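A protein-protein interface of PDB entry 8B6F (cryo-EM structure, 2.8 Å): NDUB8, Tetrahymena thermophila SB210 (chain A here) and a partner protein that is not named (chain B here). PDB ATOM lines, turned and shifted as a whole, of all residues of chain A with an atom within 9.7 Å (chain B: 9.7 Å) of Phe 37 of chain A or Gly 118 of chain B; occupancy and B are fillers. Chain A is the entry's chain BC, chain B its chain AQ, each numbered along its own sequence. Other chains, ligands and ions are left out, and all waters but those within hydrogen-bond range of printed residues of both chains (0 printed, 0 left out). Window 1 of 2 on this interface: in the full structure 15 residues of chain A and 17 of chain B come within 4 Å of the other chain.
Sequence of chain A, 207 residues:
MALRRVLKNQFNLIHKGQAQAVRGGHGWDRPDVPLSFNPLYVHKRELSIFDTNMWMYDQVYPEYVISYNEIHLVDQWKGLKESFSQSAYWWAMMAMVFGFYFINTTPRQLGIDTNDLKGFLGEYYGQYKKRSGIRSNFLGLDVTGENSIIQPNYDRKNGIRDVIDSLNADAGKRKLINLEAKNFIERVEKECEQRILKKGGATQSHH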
ATOM      1  N   ARG A  30      10.369  14.970 -31.195  1.00  0.00           N
ATOM      2  CA  ARG A  30      11.523  14.242 -30.704  1.00  0.00           C
ATOM      3  C   ARG A  30      12.247  13.493 -31.824  1.00  0.00           C
ATOM      4  O   ARG A  30      11.604  12.967 -32.737  1.00  0.00           O
ATOM      5  CB  ARG A  30      11.072  13.279 -29.612  1.00  0.00           C
ATOM      6  CG  ARG A  30      10.584  14.019 -28.375  1.00  0.00           C
ATOM      7  CD  ARG A  30       9.872  13.112 -27.396  1.00  0.00           C
ATOM      8  NE  ARG A  30      10.632  11.902 -27.115  1.00  0.00           N
ATOM      9  CZ  ARG A  30      11.690  11.854 -26.319  1.00  0.00           C
ATOM     10  NH1 ARG A  30      12.140  12.934 -25.702  1.00  0.00           N
ATOM     11  NH2 ARG A  30      12.309  10.694 -26.134  1.00  0.00           N
ATOM     12  N   ASP A  32      14.260  10.321 -33.562  1.00  0.00           N
ATOM     13  CA  ASP A  32      13.902   8.907 -33.481  1.00  0.00           C
ATOM     14  C   ASP A  32      14.724   8.233 -32.387  1.00  0.00           C
ATOM     15  O   ASP A  32      15.843   8.654 -32.083  1.00  0.00           O
ATOM     16  CB  ASP A  32      14.149   8.200 -34.812  1.00  0.00           C
ATOM     17  CG  ASP A  32      12.890   8.054 -35.640  1.00  0.00           C
ATOM     18  OD1 ASP A  32      11.957   8.862 -35.455  1.00  0.00           O
ATOM     19  OD2 ASP A  32      12.832   7.126 -36.475  1.00  0.00           O
ATOM     20  N   VAL A  33      14.163   7.187 -31.779  1.00  0.00           N
ATOM     21  CA  VAL A  33      14.731   6.651 -30.543  1.00  0.00           C
ATOM     22  C   VAL A  33      16.210   6.355 -30.760  1.00  0.00           C
ATOM     23  O   VAL A  33      16.593   5.772 -31.784  1.00  0.00           O
ATOM     24  CB  VAL A  33      13.988   5.372 -30.111  1.00  0.00           C
ATOM     25  CG1 VAL A  33      14.731   4.628 -28.999  1.00  0.00           C
ATOM     26  CG2 VAL A  33      12.565   5.687 -29.682  1.00  0.00           C
ATOM     27  N   PRO A  34      17.068   6.744 -29.818  1.00  0.00           N
ATOM     28  CA  PRO A  34      18.513   6.604 -30.023  1.00  0.00           C
ATOM     29  C   PRO A  34      19.022   5.174 -30.073  1.00  0.00           C
ATOM     30  O   PRO A  34      18.553   4.298 -29.343  1.00  0.00           O
ATOM     31  CB  PRO A  34      19.102   7.343 -28.816  1.00  0.00           C
ATOM     32  CG  PRO A  34      18.068   7.205 -27.773  1.00  0.00           C
ATOM     33  CD  PRO A  34      16.770   7.337 -28.501  1.00  0.00           C
ATOM     34  N   LEU A  35      19.998   4.949 -30.951  1.00  0.00           N
ATOM     35  CA  LEU A  35      20.658   3.652 -31.034  1.00  0.00           C
ATOM     36  C   LEU A  35      21.477   3.439 -29.765  1.00  0.00           C
ATOM     37  O   LEU A  35      21.833   2.304 -29.431  1.00  0.00           O
ATOM     38  CB  LEU A  35      21.496   3.541 -32.305  1.00  0.00           C
ATOM     39  CG  LEU A  35      20.620   3.163 -33.506  1.00  0.00           C
ATOM     40  CD1 LEU A  35      21.207   3.661 -34.811  1.00  0.00           C
ATOM     41  CD2 LEU A  35      20.399   1.657 -33.565  1.00  0.00           C
ATOM     42  N   SER A  36      21.765   4.546 -29.070  1.00  0.00           N
ATOM     43  CA  SER A  36      22.492   4.598 -27.805  1.00  0.00           C
ATOM     44  C   SER A  36      21.719   3.894 -26.702  1.00  0.00           C
ATOM     45  O   SER A  36      22.312   3.521 -25.682  1.00  0.00           O
ATOM     46  CB  SER A  36      22.784   6.046 -27.411  1.00  0.00           C
ATOM     47  OG  SER A  36      21.868   6.510 -26.435  1.00  0.00           O
ATOM     48  N   PHE A  37      20.410   3.717 -26.880  1.00  0.00           N
ATOM     49  CA  PHE A  37      19.597   3.074 -25.857  1.00  0.00           C
ATOM     50  C   PHE A  37      20.152   1.678 -25.614  1.00  0.00           C
ATOM     51  O   PHE A  37      20.226   1.224 -24.466  1.00  0.00           O
ATOM     52  CB  PHE A  37      18.137   3.059 -26.328  1.00  0.00           C
ATOM     53  CG  PHE A  37      17.188   2.289 -25.447  1.00  0.00           C
ATOM     54  CD1 PHE A  37      17.116   0.907 -25.512  1.00  0.00           C
ATOM     55  CD2 PHE A  37      16.329   2.958 -24.591  1.00  0.00           C
ATOM     56  CE1 PHE A  37      16.224   0.207 -24.718  1.00  0.00           C
ATOM     57  CE2 PHE A  37      15.440   2.264 -23.793  1.00  0.00           C
ATOM     58  CZ  PHE A  37      15.387   0.887 -23.858  1.00  0.00           C
ATOM     59  N   ASN A  38      20.549   0.982 -26.677  1.00  0.00           N
ATOM     60  CA  ASN A  38      21.282  -0.259 -26.493  1.00  0.00           C
ATOM     61  C   ASN A  38      22.733   0.103 -26.789  1.00  0.00           C
ATOM     62  O   ASN A  38      23.081   0.326 -27.958  1.00  0.00           O
ATOM     63  CB  ASN A  38      20.786  -1.352 -27.432  1.00  0.00           C
ATOM     64  CG  ASN A  38      19.291  -1.550 -27.338  1.00  0.00           C
ATOM     65  OD1 ASN A  38      18.574  -1.440 -28.330  1.00  0.00           O
ATOM     66  ND2 ASN A  38      18.807  -1.813 -26.129  1.00  0.00           N
ATOM     67  N   PRO A  39      23.610   0.173 -25.771  1.00  0.00           N
ATOM     68  CA  PRO A  39      25.041   0.446 -25.996  1.00  0.00           C
ATOM     69  C   PRO A  39      25.925  -0.755 -26.280  1.00  0.00           C
ATOM     70  O   PRO A  39      25.941  -1.696 -25.484  1.00  0.00           O
ATOM     71  CB  PRO A  39      25.461   1.100 -24.676  1.00  0.00           C
ATOM     72  CG  PRO A  39      24.597   0.433 -23.677  1.00  0.00           C
ATOM     73  CD  PRO A  39      23.262   0.280 -24.343  1.00  0.00           C
ATOM     74  N   LEU A  40      26.664  -0.754 -27.388  1.00  0.00           N
ATOM     75  CA  LEU A  40      27.492  -1.912 -27.689  1.00  0.00           C
ATOM     76  C   LEU A  40      28.529  -2.091 -26.590  1.00  0.00           C
ATOM     77  O   LEU A  40      29.176  -1.132 -26.165  1.00  0.00           O
ATOM     78  CB  LEU A  40      28.188  -1.731 -29.039  1.00  0.00           C
ATOM     79  CG  LEU A  40      29.085  -2.889 -29.486  1.00  0.00           C
ATOM     80  CD1 LEU A  40      28.286  -4.166 -29.672  1.00  0.00           C
ATOM     81  CD2 LEU A  40      29.832  -2.533 -30.762  1.00  0.00           C
ATOM     82  N   ASP A  58      26.290 -11.281 -22.977  1.00  0.00           N
ATOM     83  CA  ASP A  58      25.436 -10.402 -23.758  1.00  0.00           C
ATOM     84  C   ASP A  58      26.317  -9.425 -24.519  1.00  0.00           C
ATOM     85  O   ASP A  58      27.471  -9.190 -24.155  1.00  0.00           O
ATOM     86  CB  ASP A  58      24.440  -9.650 -22.871  1.00  0.00           C
ATOM     87  CG  ASP A  58      23.380  -8.926 -23.672  1.00  0.00           C
ATOM     88  OD1 ASP A  58      23.362  -9.083 -24.908  1.00  0.00           O
ATOM     89  OD2 ASP A  58      22.564  -8.201 -23.067  1.00  0.00           O
ATOM     90  N   GLN A  59      25.761  -8.862 -25.586  1.00  0.00           N
ATOM     91  CA  GLN A  59      26.474  -7.900 -26.413  1.00  0.00           C
ATOM     92  C   GLN A  59      26.193  -6.457 -26.021  1.00  0.00           C
ATOM     93  O   GLN A  59      26.785  -5.548 -26.610  1.00  0.00           O
ATOM     94  CB  GLN A  59      26.115  -8.112 -27.886  1.00  0.00           C
ATOM     95  CG  GLN A  59      26.426  -9.511 -28.388  1.00  0.00           C
ATOM     96  CD  GLN A  59      26.073  -9.697 -29.843  1.00  0.00           C
ATOM     97  OE1 GLN A  59      25.728  -8.744 -30.537  1.00  0.00           O
ATOM     98  NE2 GLN A  59      26.155 -10.935 -30.317  1.00  0.00           N
ATOM     99  N   VAL A  60      25.314  -6.223 -25.049  1.00  0.00           N
ATOM    100  CA  VAL A  60      24.977  -4.869 -24.625  1.00  0.00           C
ATOM    101  C   VAL A  60      25.205  -4.732 -23.127  1.00  0.00           C
ATOM    102  O   VAL A  60      25.962  -3.865 -22.679  1.00  0.00           O
ATOM    103  CB  VAL A  60      23.524  -4.521 -25.000  1.00  0.00           C
ATOM    104  CG1 VAL A  60      23.156  -3.133 -24.508  1.00  0.00           C
ATOM    105  CG2 VAL A  60      23.330  -4.619 -26.499  1.00  0.00           C
ATOM    106  N   TYR A  61      24.554  -5.588 -22.341  1.00  0.00           N
ATOM    107  CA  TYR A  61      24.612  -5.536 -20.880  1.00  0.00           C
ATOM    108  C   TYR A  61      24.915  -6.925 -20.335  1.00  0.00           C
ATOM    109  O   TYR A  61      24.038  -7.591 -19.774  1.00  0.00           O
ATOM    110  CB  TYR A  61      23.300  -5.005 -20.302  1.00  0.00           C
ATOM    111  CG  TYR A  61      23.026  -3.546 -20.594  1.00  0.00           C
ATOM    112  CD1 TYR A  61      24.046  -2.603 -20.558  1.00  0.00           C
ATOM    113  CD2 TYR A  61      21.745  -3.113 -20.902  1.00  0.00           C
ATOM    114  CE1 TYR A  61      23.797  -1.272 -20.822  1.00  0.00           C
ATOM    115  CE2 TYR A  61      21.486  -1.786 -21.168  1.00  0.00           C
ATOM    116  CZ  TYR A  61      22.515  -0.870 -21.127  1.00  0.00           C
ATOM    117  OH  TYR A  61      22.256   0.455 -21.391  1.00  0.00           O
ATOM    118  N   GLU A  63      26.059  -9.718 -17.741  1.00  0.00           N
ATOM    119  CA  GLU A  63      25.820  -9.769 -16.309  1.00  0.00           C
ATOM    120  C   GLU A  63      26.376 -11.063 -15.736  1.00  0.00           C
ATOM    121  O   GLU A  63      26.477 -12.075 -16.432  1.00  0.00           O
ATOM    122  CB  GLU A  63      24.323  -9.670 -15.990  1.00  0.00           C
ATOM    123  CG  GLU A  63      23.677  -8.393 -16.494  1.00  0.00           C
ATOM    124  CD  GLU A  63      22.234  -8.261 -16.060  1.00  0.00           C
ATOM    125  OE1 GLU A  63      21.815  -9.016 -15.158  1.00  0.00           O
ATOM    126  OE2 GLU A  63      21.518  -7.406 -16.621  1.00  0.00           O
ATOM    127  N   GLU B 109      15.542   4.884 -13.898  1.00  0.00           N
ATOM    128  CA  GLU B 109      15.430   4.193 -15.175  1.00  0.00           C
ATOM    129  C   GLU B 109      16.315   4.797 -16.255  1.00  0.00           C
ATOM    130  O   GLU B 109      16.472   4.185 -17.316  1.00  0.00           O
ATOM    131  CB  GLU B 109      13.976   4.208 -15.651  1.00  0.00           C
ATOM    132  CG  GLU B 109      12.951   3.784 -14.601  1.00  0.00           C
ATOM    133  CD  GLU B 109      13.075   2.327 -14.191  1.00  0.00           C
ATOM    134  OE1 GLU B 109      14.210   1.829 -14.052  1.00  0.00           O
ATOM    135  OE2 GLU B 109      12.028   1.674 -14.005  1.00  0.00           O
ATOM    136  N   SER B 110      16.895   5.968 -16.015  1.00  0.00           N
ATOM    137  CA  SER B 110      17.748   6.627 -16.994  1.00  0.00           C
ATOM    138  C   SER B 110      19.190   6.143 -16.950  1.00  0.00           C
ATOM    139  O   SER B 110      20.009   6.623 -17.741  1.00  0.00           O
ATOM    140  CB  SER B 110      17.700   8.139 -16.775  1.00  0.00           C
ATOM    141  OG  SER B 110      18.283   8.485 -15.535  1.00  0.00           O
ATOM    142  N   ARG B 111      19.519   5.227 -16.056  1.00  0.00           N
ATOM    143  CA  ARG B 111      20.881   4.748 -15.915  1.00  0.00           C
ATOM    144  C   ARG B 111      21.042   3.369 -16.544  1.00  0.00           C
ATOM    145  O   ARG B 111      20.089   2.587 -16.593  1.00  0.00           O
ATOM    146  CB  ARG B 111      21.255   4.679 -14.435  1.00  0.00           C
ATOM    147  CG  ARG B 111      21.188   6.020 -13.730  1.00  0.00           C
ATOM    148  CD  ARG B 111      21.332   5.839 -12.243  1.00  0.00           C
ATOM    149  NE  ARG B 111      22.600   5.207 -11.919  1.00  0.00           N
ATOM    150  CZ  ARG B 111      22.994   4.900 -10.693  1.00  0.00           C
ATOM    151  NH1 ARG B 111      22.238   5.156  -9.638  1.00  0.00           N
ATOM    152  NH2 ARG B 111      24.163   4.294 -10.525  1.00  0.00           N
ATOM    153  N   PRO B 112      22.234   3.031 -17.039  1.00  0.00           N
ATOM    154  CA  PRO B 112      22.449   1.683 -17.571  1.00  0.00           C
ATOM    155  C   PRO B 112      22.257   0.619 -16.503  1.00  0.00           C
ATOM    156  O   PRO B 112      22.291   0.888 -15.302  1.00  0.00           O
ATOM    157  CB  PRO B 112      23.899   1.720 -18.065  1.00  0.00           C
ATOM    158  CG  PRO B 112      24.184   3.152 -18.305  1.00  0.00           C
ATOM    159  CD  PRO B 112      23.396   3.906 -17.281  1.00  0.00           C
ATOM    160  N   TYR B 113      22.028  -0.608 -16.963  1.00  0.00           N
ATOM    161  CA  TYR B 113      21.858  -1.784 -16.114  1.00  0.00           C
ATOM    162  C   TYR B 113      20.685  -1.659 -15.152  1.00  0.00           C
ATOM    163  O   TYR B 113      20.544  -2.490 -14.248  1.00  0.00           O
ATOM    164  CB  TYR B 113      23.135  -2.091 -15.325  1.00  0.00           C
ATOM    165  CG  TYR B 113      24.290  -2.554 -16.180  1.00  0.00           C
ATOM    166  CD1 TYR B 113      24.469  -3.899 -16.467  1.00  0.00           C
ATOM    167  CD2 TYR B 113      25.209  -1.647 -16.689  1.00  0.00           C
ATOM    168  CE1 TYR B 113      25.524  -4.329 -17.243  1.00  0.00           C
ATOM    169  CE2 TYR B 113      26.268  -2.067 -17.466  1.00  0.00           C
ATOM    170  CZ  TYR B 113      26.420  -3.409 -17.739  1.00  0.00           C
ATOM    171  OH  TYR B 113      27.473  -3.833 -18.513  1.00  0.00           O
ATOM    172  N   ALA B 114      19.843  -0.645 -15.313  1.00  0.00           N
ATOM    173  CA  ALA B 114      18.675  -0.507 -14.461  1.00  0.00           C
ATOM    174  C   ALA B 114      17.537  -1.377 -14.981  1.00  0.00           C
ATOM    175  O   ALA B 114      17.559  -1.863 -16.113  1.00  0.00           O
ATOM    176  CB  ALA B 114      18.229   0.952 -14.392  1.00  0.00           C
ATOM    177  N   ALA B 115      16.539  -1.583 -14.129  1.00  0.00           N
ATOM    178  CA  ALA B 115      15.336  -2.271 -14.568  1.00  0.00           C
ATOM    179  C   ALA B 115      14.683  -1.476 -15.691  1.00  0.00           C
ATOM    180  O   ALA B 115      14.472  -0.267 -15.569  1.00  0.00           O
ATOM    181  CB  ALA B 115      14.368  -2.445 -13.400  1.00  0.00           C
ATOM    182  N   SER B 116      14.365  -2.158 -16.788  1.00  0.00           N
ATOM    183  CA  SER B 116      13.811  -1.561 -17.999  1.00  0.00           C
ATOM    184  C   SER B 116      14.885  -0.877 -18.834  1.00  0.00           C
ATOM    185  O   SER B 116      14.551  -0.146 -19.777  1.00  0.00           O
ATOM    186  CB  SER B 116      12.700  -0.550 -17.695  1.00  0.00           C
ATOM    187  OG  SER B 116      13.214   0.595 -17.036  1.00  0.00           O
ATOM    188  N   SER B 117      16.164  -1.086 -18.521  1.00  0.00           N
ATOM    189  CA  SER B 117      17.229  -0.393 -19.237  1.00  0.00           C
ATOM    190  C   SER B 117      17.280  -0.801 -20.705  1.00  0.00           C
ATOM    191  O   SER B 117      17.439   0.051 -21.586  1.00  0.00           O
ATOM    192  CB  SER B 117      18.572  -0.667 -18.563  1.00  0.00           C
ATOM    193  OG  SER B 117      19.635  -0.080 -19.292  1.00  0.00           O
ATOM    194  N   GLY B 118      17.148  -2.094 -20.988  1.00  0.00           N
ATOM    195  CA  GLY B 118      17.331  -2.596 -22.336  1.00  0.00           C
ATOM    196  C   GLY B 118      16.165  -3.419 -22.839  1.00  0.00           C
ATOM    197  O   GLY B 118      16.357  -4.419 -23.536  1.00  0.00           O
ATOM    198  N   ARG B 119      14.946  -3.010 -22.491  1.00  0.00           N
ATOM    199  CA  ARG B 119      13.770  -3.785 -22.863  1.00  0.00           C
ATOM    200  C   ARG B 119      13.546  -3.843 -24.366  1.00  0.00           C
ATOM    201  O   ARG B 119      12.814  -4.722 -24.829  1.00  0.00           O
ATOM    202  CB  ARG B 119      12.528  -3.212 -22.187  1.00  0.00           C
ATOM    203  CG  ARG B 119      12.404  -3.595 -20.730  1.00  0.00           C
ATOM    204  CD  ARG B 119      11.274  -2.835 -20.059  1.00  0.00           C
ATOM    205  NE  ARG B 119      11.101  -3.228 -18.667  1.00  0.00           N
ATOM    206  CZ  ARG B 119      10.155  -2.753 -17.869  1.00  0.00           C
ATOM    207  NH1 ARG B 119       9.274  -1.863 -18.294  1.00  0.00           N
ATOM    208  NH2 ARG B 119      10.089  -3.183 -16.612  1.00  0.00           N
ATOM    209  N   TYR B 120      14.143  -2.939 -25.138  1.00  0.00           N
ATOM    210  CA  TYR B 120      13.867  -2.842 -26.563  1.00  0.00           C
ATOM    211  C   TYR B 120      15.167  -2.833 -27.353  1.00  0.00           C
ATOM    212  O   TYR B 120      16.161  -2.240 -26.924  1.00  0.00           O
ATOM    213  CB  TYR B 120      13.047  -1.590 -26.871  1.00  0.00           C
ATOM    214  CG  TYR B 120      11.916  -1.387 -25.892  1.00  0.00           C
ATOM    215  CD1 TYR B 120      10.720  -2.073 -26.032  1.00  0.00           C
ATOM    216  CD2 TYR B 120      12.053  -0.521 -24.817  1.00  0.00           C
ATOM    217  CE1 TYR B 120       9.687  -1.896 -25.135  1.00  0.00           C
ATOM    218  CE2 TYR B 120      11.027  -0.338 -23.913  1.00  0.00           C
ATOM    219  CZ  TYR B 120       9.847  -1.029 -24.078  1.00  0.00           C
ATOM    220  OH  TYR B 120       8.821  -0.848 -23.182  1.00  0.00           O
ATOM    221  N   TYR B 121      15.152  -3.499 -28.505  1.00  0.00           N
ATOM    222  CA  TYR B 121      16.290  -3.542 -29.412  1.00  0.00           C
ATOM    223  C   TYR B 121      16.014  -2.603 -30.579  1.00  0.00           C
ATOM    224  O   TYR B 121      15.065  -2.816 -31.341  1.00  0.00           O
ATOM    225  CB  TYR B 121      16.533  -4.967 -29.910  1.00  0.00           C
ATOM    226  CG  TYR B 121      17.574  -5.072 -31.000  1.00  0.00           C
ATOM    227  CD1 TYR B 121      18.916  -4.838 -30.736  1.00  0.00           C
ATOM    228  CD2 TYR B 121      17.212  -5.424 -32.291  1.00  0.00           C
ATOM    229  CE1 TYR B 121      19.867  -4.941 -31.732  1.00  0.00           C
ATOM    230  CE2 TYR B 121      18.155  -5.531 -33.292  1.00  0.00           C
ATOM    231  CZ  TYR B 121      19.480  -5.288 -33.006  1.00  0.00           C
ATOM    232  OH  TYR B 121      20.420  -5.393 -34.003  1.00  0.00           O
ATOM    233  N   ILE B 122      16.843  -1.575 -30.717  1.00  0.00           N
ATOM    234  CA  ILE B 122      16.655  -0.553 -31.739  1.00  0.00           C
ATOM    235  C   ILE B 122      17.365  -0.993 -33.011  1.00  0.00           C
ATOM    236  O   ILE B 122      18.557  -1.323 -32.986  1.00  0.00           O
ATOM    237  CB  ILE B 122      17.184   0.806 -31.253  1.00  0.00           C
ATOM    238  CG1 ILE B 122      16.646   1.125 -29.855  1.00  0.00           C
ATOM    239  CG2 ILE B 122      16.802   1.906 -32.227  1.00  0.00           C
ATOM    240  CD1 ILE B 122      15.139   1.093 -29.742  1.00  0.00           C
ATOM    241  N   PHE B 123      16.636  -0.997 -34.123  1.00  0.00           N
ATOM    242  CA  PHE B 123      17.186  -1.466 -35.386  1.00  0.00           C
ATOM    243  C   PHE B 123      17.951  -0.351 -36.086  1.00  0.00           C
ATOM    244  O   PHE B 123      17.484   0.788 -36.171  1.00  0.00           O
ATOM    245  CB  PHE B 123      16.070  -1.988 -36.288  1.00  0.00           C
ATOM    246  CG  PHE B 123      15.351  -3.179 -35.726  1.00  0.00           C
ATOM    247  CD1 PHE B 123      15.834  -4.458 -35.939  1.00  0.00           C
ATOM    248  CD2 PHE B 123      14.194  -3.019 -34.985  1.00  0.00           C
ATOM    249  CE1 PHE B 123      15.177  -5.557 -35.425  1.00  0.00           C
ATOM    250  CE2 PHE B 123      13.532  -4.114 -34.466  1.00  0.00           C
ATOM    251  CZ  PHE B 123      14.024  -5.385 -34.687  1.00  0.00           C
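N of Tyr 113 of chain B is in hydrogen-bond range of OG of Ser 117 of chain B.
N of Tyr 61 of chain A sits at hydrogen-bond distance from OD2 of Asp 58 of chain A, 3.4 Å away.
Pro 34 of chain A touches just one residue of chain B: Ile 122.
Of chain B, only Ser 117 (3.2 Å), Gly 118 (3.8 Å) and Tyr 120 (3.3 Å) come within 4 Å of Phe 37 of chain A.
Asn 38 of chain A touches just these residues of chain B: Tyr 120, Tyr 121 and Ile 122.
Printed residues of chain B within 4 Å of Tyr 61 of chain A: Pro 112 (3.9 Å), Tyr 113 (3.8 Å) and Ser 117 (3.1 Å).
Of the printed residues of chain A, Tyr 113 of chain B touches Tyr 61 (3.8 Å).
Ser 117 of chain B touches just these residues of chain A: Phe 37 (3.2 Å) and Tyr 61 (3.1 Å).
Gly 118 of chain B touches just one residue of chain A: Phe 37 (3.8 Å).
Of the printed residues of chain A, Ile 122 of chain B touches Val 33 (3.6 Å), Pro 34 (3.7 Å), Leu 35 (3.6 Å) and Asn 38 (3.0 Å).
Hydrophobic or aromatic side chains of chain B within 4 Å of the printed part of chain A: Pro 112, Tyr 113, Tyr 120 and Ile 122.
Printed residues of chain A that touch a printed residue of chain B: Val 33, Pro 34, Leu 35, Phe 37, Asn 38 and Tyr 61.
Hydrophobic or aromatic side chains of chain A that line the printed part of chain B: Val 33, Leu 35, Phe 37 and Tyr 61.
Among the printed residues, 12 pairs touch across the chains.
Among the printed residues, pairs that only touch across the chains: Phe 37 of chain A with Ser 117 of chain B, Asn 38 of chain A with Tyr 121 of chain B, Phe 37 of chain A with Tyr 120 of chain B, Leu 35 of chain A with Ile 122 of chain B, Val 33 of chain A with Ile 122 of chain B, Pro 34 of chain A with Ile 122 of chain B, Tyr 61 of chain A with Tyr 113 of chain B, Phe 37 of chain A with Gly 118 of chain B and Tyr 61 of chain A with Pro 112 of chain B.
The side-chain hydroxyl of Ser 117 of chain B lies close to the side-chain hydroxyl of Tyr 61 of chain A (3.4 Å).
The backbone carbonyl oxygen of Tyr 120 of chain B is in hydrogen-bond range of the side-chain amide nitrogen of Asn 38 of chain A.
The backbone NH of Ile 122 of chain B is in hydrogen-bond range of the side-chain amide oxygen of Asn 38 of chain A.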
